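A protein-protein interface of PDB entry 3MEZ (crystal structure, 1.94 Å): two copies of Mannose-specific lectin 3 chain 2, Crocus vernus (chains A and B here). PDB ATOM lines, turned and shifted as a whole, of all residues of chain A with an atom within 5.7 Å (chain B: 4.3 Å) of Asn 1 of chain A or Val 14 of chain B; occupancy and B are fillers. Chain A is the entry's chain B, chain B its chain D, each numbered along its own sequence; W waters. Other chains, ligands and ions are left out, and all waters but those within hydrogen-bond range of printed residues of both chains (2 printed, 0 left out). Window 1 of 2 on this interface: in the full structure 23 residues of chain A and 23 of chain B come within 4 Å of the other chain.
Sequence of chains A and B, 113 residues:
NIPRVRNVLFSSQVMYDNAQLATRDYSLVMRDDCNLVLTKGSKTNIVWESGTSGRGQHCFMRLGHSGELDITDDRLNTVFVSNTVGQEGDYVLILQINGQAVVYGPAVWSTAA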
ATOM      1  N   ASN A   1       9.414  -0.764  -1.851  1.00  0.00           N
ATOM      2  CA  ASN A   1       8.411   0.087  -2.446  1.00  0.00           C
ATOM      3  C   ASN A   1       8.004   1.265  -1.586  1.00  0.00           C
ATOM      4  O   ASN A   1       7.660   1.122  -0.463  1.00  0.00           O
ATOM      5  CB  ASN A   1       7.205  -0.720  -2.847  1.00  0.00           C
ATOM      6  CG  ASN A   1       7.495  -1.669  -3.970  1.00  0.00           C
ATOM      7  OD1 ASN A   1       8.493  -2.267  -3.996  1.00  0.00           O
ATOM      8  ND2 ASN A   1       6.605  -1.747  -4.916  1.00  0.00           N
ATOM      9  N   ILE A   2       8.070   2.424  -2.195  1.00  0.00           N
ATOM     10  CA  ILE A   2       7.709   3.685  -1.597  1.00  0.00           C
ATOM     11  C   ILE A   2       6.236   3.983  -1.897  1.00  0.00           C
ATOM     12  O   ILE A   2       5.796   3.827  -2.962  1.00  0.00           O
ATOM     13  CB  ILE A   2       8.620   4.824  -2.142  1.00  0.00           C
ATOM     14  CG1 ILE A   2      10.083   4.527  -1.920  1.00  0.00           C
ATOM     15  CG2 ILE A   2       8.278   6.138  -1.565  1.00  0.00           C
ATOM     16  CD1 ILE A   2      10.952   5.231  -2.843  1.00  0.00           C
ATOM     17  N   PRO A   3       5.501   4.437  -0.912  1.00  0.00           N
ATOM     18  CA  PRO A   3       4.093   4.745  -1.091  1.00  0.00           C
ATOM     19  C   PRO A   3       3.880   5.858  -2.140  1.00  0.00           C
ATOM     20  O   PRO A   3       4.705   6.679  -2.281  1.00  0.00           O
ATOM     21  CB  PRO A   3       3.702   5.229   0.275  1.00  0.00           C
ATOM     22  CG  PRO A   3       4.566   4.612   1.151  1.00  0.00           C
ATOM     23  CD  PRO A   3       5.869   4.497   0.492  1.00  0.00           C
ATOM     24  N   SER A  12      13.052   5.119  -8.260  1.00  0.00           N
ATOM     25  CA  SER A  12      12.602   3.729  -8.276  1.00  0.00           C
ATOM     26  C   SER A  12      11.069   3.576  -8.462  1.00  0.00           C
ATOM     27  O   SER A  12      10.622   2.575  -8.879  1.00  0.00           O
ATOM     28  CB  SER A  12      13.082   2.931  -7.051  1.00  0.00           C
ATOM     29  OG  SER A  12      14.432   2.621  -7.059  1.00  0.00           O
ATOM     30  N   VAL A  14       7.445   4.077 -10.315  1.00  0.00           N
ATOM     31  CA  VAL A  14       6.978   4.000 -11.673  1.00  0.00           C
ATOM     32  C   VAL A  14       5.525   4.465 -11.834  1.00  0.00           C
ATOM     33  O   VAL A  14       4.783   4.427 -10.928  1.00  0.00           O
ATOM     34  CB  VAL A  14       7.078   2.572 -12.225  1.00  0.00           C
ATOM     35  CG1 VAL A  14       8.444   2.075 -12.191  1.00  0.00           C
ATOM     36  CG2 VAL A  14       6.190   1.671 -11.468  1.00  0.00           C
ATOM     37  N   TYR A  16       2.231   3.987 -14.703  1.00  0.00           N
ATOM     38  CA  TYR A  16       1.734   3.355 -15.891  1.00  0.00           C
ATOM     39  C   TYR A  16       0.214   3.379 -16.015  1.00  0.00           C
ATOM     40  O   TYR A  16      -0.477   3.572 -15.062  1.00  0.00           O
ATOM     41  CB  TYR A  16       2.288   1.942 -16.012  1.00  0.00           C
ATOM     42  CG  TYR A  16       2.006   1.073 -14.833  1.00  0.00           C
ATOM     43  CD1 TYR A  16       2.891   0.975 -13.805  1.00  0.00           C
ATOM     44  CD2 TYR A  16       0.840   0.381 -14.737  1.00  0.00           C
ATOM     45  CE1 TYR A  16       2.648   0.228 -12.737  1.00  0.00           C
ATOM     46  CE2 TYR A  16       0.573  -0.380 -13.667  1.00  0.00           C
ATOM     47  CZ  TYR A  16       1.471  -0.463 -12.665  1.00  0.00           C
ATOM     48  OH  TYR A  16       1.179  -1.215 -11.618  1.00  0.00           O
ATOM     49  N   ARG B   4      -1.043  -2.525  -4.614  1.00  0.00           N
ATOM     50  CA  ARG B   4      -0.208  -3.581  -4.081  1.00  0.00           C
ATOM     51  C   ARG B   4      -1.050  -4.598  -3.306  1.00  0.00           C
ATOM     52  O   ARG B   4      -1.935  -4.247  -2.600  1.00  0.00           O
ATOM     53  CB  ARG B   4       0.935  -2.971  -3.254  1.00  0.00           C
ATOM     54  CG  ARG B   4       2.074  -2.377  -4.108  1.00  0.00           C
ATOM     55  CD  ARG B   4       2.685  -0.987  -3.773  1.00  0.00           C
ATOM     56  NE  ARG B   4       3.501  -0.551  -4.917  1.00  0.00           N
ATOM     57  CZ  ARG B   4       4.196   0.578  -5.083  1.00  0.00           C
ATOM     58  NH1 ARG B   4       4.216   1.574  -4.197  1.00  0.00           N
ATOM     59  NH2 ARG B   4       4.878   0.734  -6.209  1.00  0.00           N
ATOM     60  N   SER B  12       2.876  -5.453 -14.953  1.00  0.00           N
ATOM     61  CA  SER B  12       3.247  -4.062 -14.819  1.00  0.00           C
ATOM     62  C   SER B  12       3.737  -3.678 -13.411  1.00  0.00           C
ATOM     63  O   SER B  12       4.354  -2.699 -13.248  1.00  0.00           O
ATOM     64  CB  SER B  12       2.137  -3.128 -15.271  1.00  0.00           C
ATOM     65  OG  SER B  12       1.992  -3.100 -16.639  1.00  0.00           O
ATOM     66  N   GLN B  13       3.416  -4.482 -12.417  1.00  0.00           N
ATOM     67  CA  GLN B  13       3.868  -4.249 -11.077  1.00  0.00           C
ATOM     68  C   GLN B  13       5.349  -4.491 -10.915  1.00  0.00           C
ATOM     69  O   GLN B  13       5.914  -5.222 -11.608  1.00  0.00           O
ATOM     70  CB  GLN B  13       3.052  -5.005 -10.024  1.00  0.00           C
ATOM     71  CG  GLN B  13       1.657  -4.480  -9.859  1.00  0.00           C
ATOM     72  CD  GLN B  13       0.881  -5.044  -8.676  1.00  0.00           C
ATOM     73  OE1 GLN B  13       0.921  -6.173  -8.419  1.00  0.00           O
ATOM     74  NE2 GLN B  13       0.176  -4.209  -7.999  1.00  0.00           N
ATOM     75  N   VAL B  14       5.905  -3.838  -9.945  1.00  0.00           N
ATOM     76  CA  VAL B  14       7.294  -3.777  -9.680  1.00  0.00           C
ATOM     77  C   VAL B  14       7.597  -3.968  -8.170  1.00  0.00           C
ATOM     78  O   VAL B  14       6.821  -3.625  -7.360  1.00  0.00           O
ATOM     79  CB  VAL B  14       7.706  -2.396 -10.180  1.00  0.00           C
ATOM     80  CG1 VAL B  14       8.180  -1.497  -9.097  1.00  0.00           C
ATOM     81  CG2 VAL B  14       8.519  -2.480 -11.318  1.00  0.00           C
ATOM     82  N   MET B  15       8.731  -4.551  -7.830  1.00  0.00           N
ATOM     83  CA  MET B  15       9.194  -4.650  -6.456  1.00  0.00           C
ATOM     84  C   MET B  15      10.643  -4.224  -6.311  1.00  0.00           C
ATOM     85  O   MET B  15      11.416  -4.533  -7.133  1.00  0.00           O
ATOM     86  CB  MET B  15       9.034  -6.072  -5.905  1.00  0.00           C
ATOM     87  CG  MET B  15       7.729  -6.757  -6.176  1.00  0.00           C
ATOM     88  SD  MET B  15       7.717  -8.476  -5.563  1.00  0.00           S
ATOM     89  CE  MET B  15       7.526  -8.016  -3.942  1.00  0.00           C
ATOM     90  N   TYR B  16      10.977  -3.519  -5.244  1.00  0.00           N
ATOM     91  CA  TYR B  16      12.329  -3.046  -5.039  1.00  0.00           C
ATOM     92  C   TYR B  16      12.631  -2.765  -3.579  1.00  0.00           C
ATOM     93  O   TYR B  16      11.761  -2.620  -2.805  1.00  0.00           O
ATOM     94  CB  TYR B  16      12.612  -1.804  -5.912  1.00  0.00           C
ATOM     95  CG  TYR B  16      11.645  -0.670  -5.705  1.00  0.00           C
ATOM     96  CD1 TYR B  16      11.823   0.241  -4.717  1.00  0.00           C
ATOM     97  CD2 TYR B  16      10.551  -0.536  -6.507  1.00  0.00           C
ATOM     98  CE1 TYR B  16      10.959   1.226  -4.529  1.00  0.00           C
ATOM     99  CE2 TYR B  16       9.683   0.439  -6.346  1.00  0.00           C
ATOM    100  CZ  TYR B  16       9.868   1.337  -5.351  1.00  0.00           C
ATOM    101  OH  TYR B  16       8.976   2.320  -5.172  1.00  0.00           O
ATOM    102  N   ALA B  19      10.974  -4.932  -0.722  1.00  0.00           N
ATOM    103  CA  ALA B  19       9.559  -5.228  -0.848  1.00  0.00           C
ATOM    104  C   ALA B  19       9.395  -6.726  -1.031  1.00  0.00           C
ATOM    105  O   ALA B  19      10.266  -7.380  -1.488  1.00  0.00           O
ATOM    106  CB  ALA B  19       8.968  -4.494  -1.992  1.00  0.00           C
ATOM    107  N   PHE B  60      15.222  -3.609  -9.528  1.00  0.00           N
ATOM    108  CA  PHE B  60      13.849  -3.876  -9.333  1.00  0.00           C
ATOM    109  C   PHE B  60      13.424  -5.150 -10.048  1.00  0.00           C
ATOM    110  O   PHE B  60      14.009  -5.498 -10.996  1.00  0.00           O
ATOM    111  CB  PHE B  60      12.981  -2.685  -9.731  1.00  0.00           C
ATOM    112  CG  PHE B  60      12.995  -2.323 -11.196  1.00  0.00           C
ATOM    113  CD1 PHE B  60      11.964  -2.645 -12.010  1.00  0.00           C
ATOM    114  CD2 PHE B  60      13.982  -1.552 -11.720  1.00  0.00           C
ATOM    115  CE1 PHE B  60      11.941  -2.255 -13.316  1.00  0.00           C
ATOM    116  CE2 PHE B  60      13.946  -1.165 -13.035  1.00  0.00           C
ATOM    117  CZ  PHE B  60      12.935  -1.521 -13.813  1.00  0.00           C
ATOM    118  N   MET B  61      12.394  -5.807  -9.547  1.00  0.00           N
ATOM    119  CA  MET B  61      11.776  -6.893 -10.245  1.00  0.00           C
ATOM    120  C   MET B  61      10.443  -6.489 -10.859  1.00  0.00           C
ATOM    121  O   MET B  61       9.708  -5.801 -10.271  1.00  0.00           O
ATOM    122  CB  MET B  61      11.571  -8.080  -9.353  1.00  0.00           C
ATOM    123  CG  MET B  61      11.345  -9.297 -10.124  1.00  0.00           C
ATOM    124  SD  MET B  61       9.648  -9.534 -10.481  1.00  0.00           S
ATOM    125  CE  MET B  61       9.052 -10.211  -8.982  1.00  0.00           C
ATOM    126  N   ARG B  62      10.207  -6.916 -12.080  1.00  0.00           N
ATOM    127  CA  ARG B  62       8.996  -6.601 -12.791  1.00  0.00           C
ATOM    128  C   ARG B  62       8.385  -7.812 -13.495  1.00  0.00           C
ATOM    129  O   ARG B  62       9.085  -8.548 -14.105  1.00  0.00           O
ATOM    130  CB  ARG B  62       9.229  -5.458 -13.794  1.00  0.00           C
ATOM    131  CG  ARG B  62       8.020  -5.090 -14.633  1.00  0.00           C
ATOM    132  CD  ARG B  62       8.341  -4.057 -15.692  1.00  0.00           C
ATOM    133  NE  ARG B  62       7.241  -3.649 -16.526  1.00  0.00           N
ATOM    134  CZ  ARG B  62       6.904  -4.255 -17.639  1.00  0.00           C
ATOM    135  NH1 ARG B  62       7.574  -5.297 -18.039  1.00  0.00           N
ATOM    136  NH2 ARG B  62       5.904  -3.833 -18.339  1.00  0.00           N
HETATM  137  O   HOH W   1       6.578   2.449  -7.345  1.00  0.00           O
HETATM  138  O   HOH W   2       4.155  -3.706  -6.362  1.00  0.00           O
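The backbone carbonyl oxygen (O) of Met 15 of chain B is in hydrogen-bond range of the backbone NH (N) of Met 61 of chain B (2.9 Å).
Asn 1 of chain A touches five residues of chain B. Pro 3 of chain A touches none of the printed residues of chain B. Of the printed residues of chain B, Ser 12 of chain A touches Tyr 16 (3.4 Å). Val 14 of chain A touches none of the printed residues of chain B. Of the printed residues of chain A, Arg 4 of chain B touches Asn 1 (3.3 Å) and Ile 2 (3.0 Å). Val 14 of chain B touches just one residue of chain A: Asn 1. The nearest printed residue of chain B that does not touch Asn 1 of chain A is Gln 13 of chain B (6.7 Å).
Among the printed residues, merely in contact across the chains: Asn 1 of chain A with Met 15 of chain B (3.5 Å), Asn 1 of chain A with Ala 19 of chain B (3.0 Å), Ser 12 of chain A with Tyr 16 of chain B (3.4 Å), Tyr 16 of chain A with Ser 12 of chain B (3.4 Å) and Tyr 16 of chain A with Gln 13 of chain B (3.7 Å).
Water W1 lies within hydrogen-bond range of the guanidinium group (NH2) of Arg 4 of chain B (2.7 Å), the side-chain hydroxyl (OH) of Tyr 16 of chain B (3.2 Å) and the backbone NH (N) of Val 14 of chain A (3.5 Å). Water W2 lies within hydrogen-bond range of the backbone carbonyl oxygen (O) of Val 14 of chain B (2.8 Å) and the side-chain amide nitrogen (ND2) of Asn 1 of chain A (3.5 Å).
Of the 10 printed residues of chain B, 7 touch a printed residue of chain A. Printed residues of chain B that touch a printed residue of chain A: Arg 4, Ser 12, Gln 13, Val 14, Met 15, Tyr 16 and Ala 19. Hydrophobic or aromatic side chains of chain B that line the printed part of chain A: Tyr 16 and Ala 19. Along chain B the printed residues that touch a printed residue of chain A span positions 4 to 19. Of the 6 printed residues of chain A, 4 touch a printed residue of chain B. Printed residues of chain A that touch a printed residue of chain B: Asn 1, Ile 2, Ser 12 and Tyr 16. Hydrophobic or aromatic side chains of chain A that line the printed part of chain B: Ile 2 and Tyr 16.
Ser 12 of chain A touches Tyr 16 of chain B, and with the chains exchanged Tyr 16 of chain A touches Ser 12 of chain B.
The guanidinium group of Arg 4 of chain B lies close to the side-chain amide nitrogen of Asn 1 of chain A, 3.3 Å away. The side-chain amide nitrogen of Asn 1 of chain A is in hydrogen-bond range of the backbone carbonyl oxygen of Val 14 of chain B (3.1 Å). The side-chain amide oxygen of Asn 1 of chain A is in hydrogen-bond range of the backbone NH of Tyr 16 of chain B, at 3.0 Å. The backbone carbonyl oxygen (O) of Ile 2 of chain A sits at hydrogen-bond distance from the guanidinium group (NH1) of Arg 4 of chain B (3.0 Å). The backbone NH (N) of Ile 2 of chain A sits at hydrogen-bond distance from the side-chain hydroxyl (OH) of Tyr 16 of chain B, 3.1 Å away.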
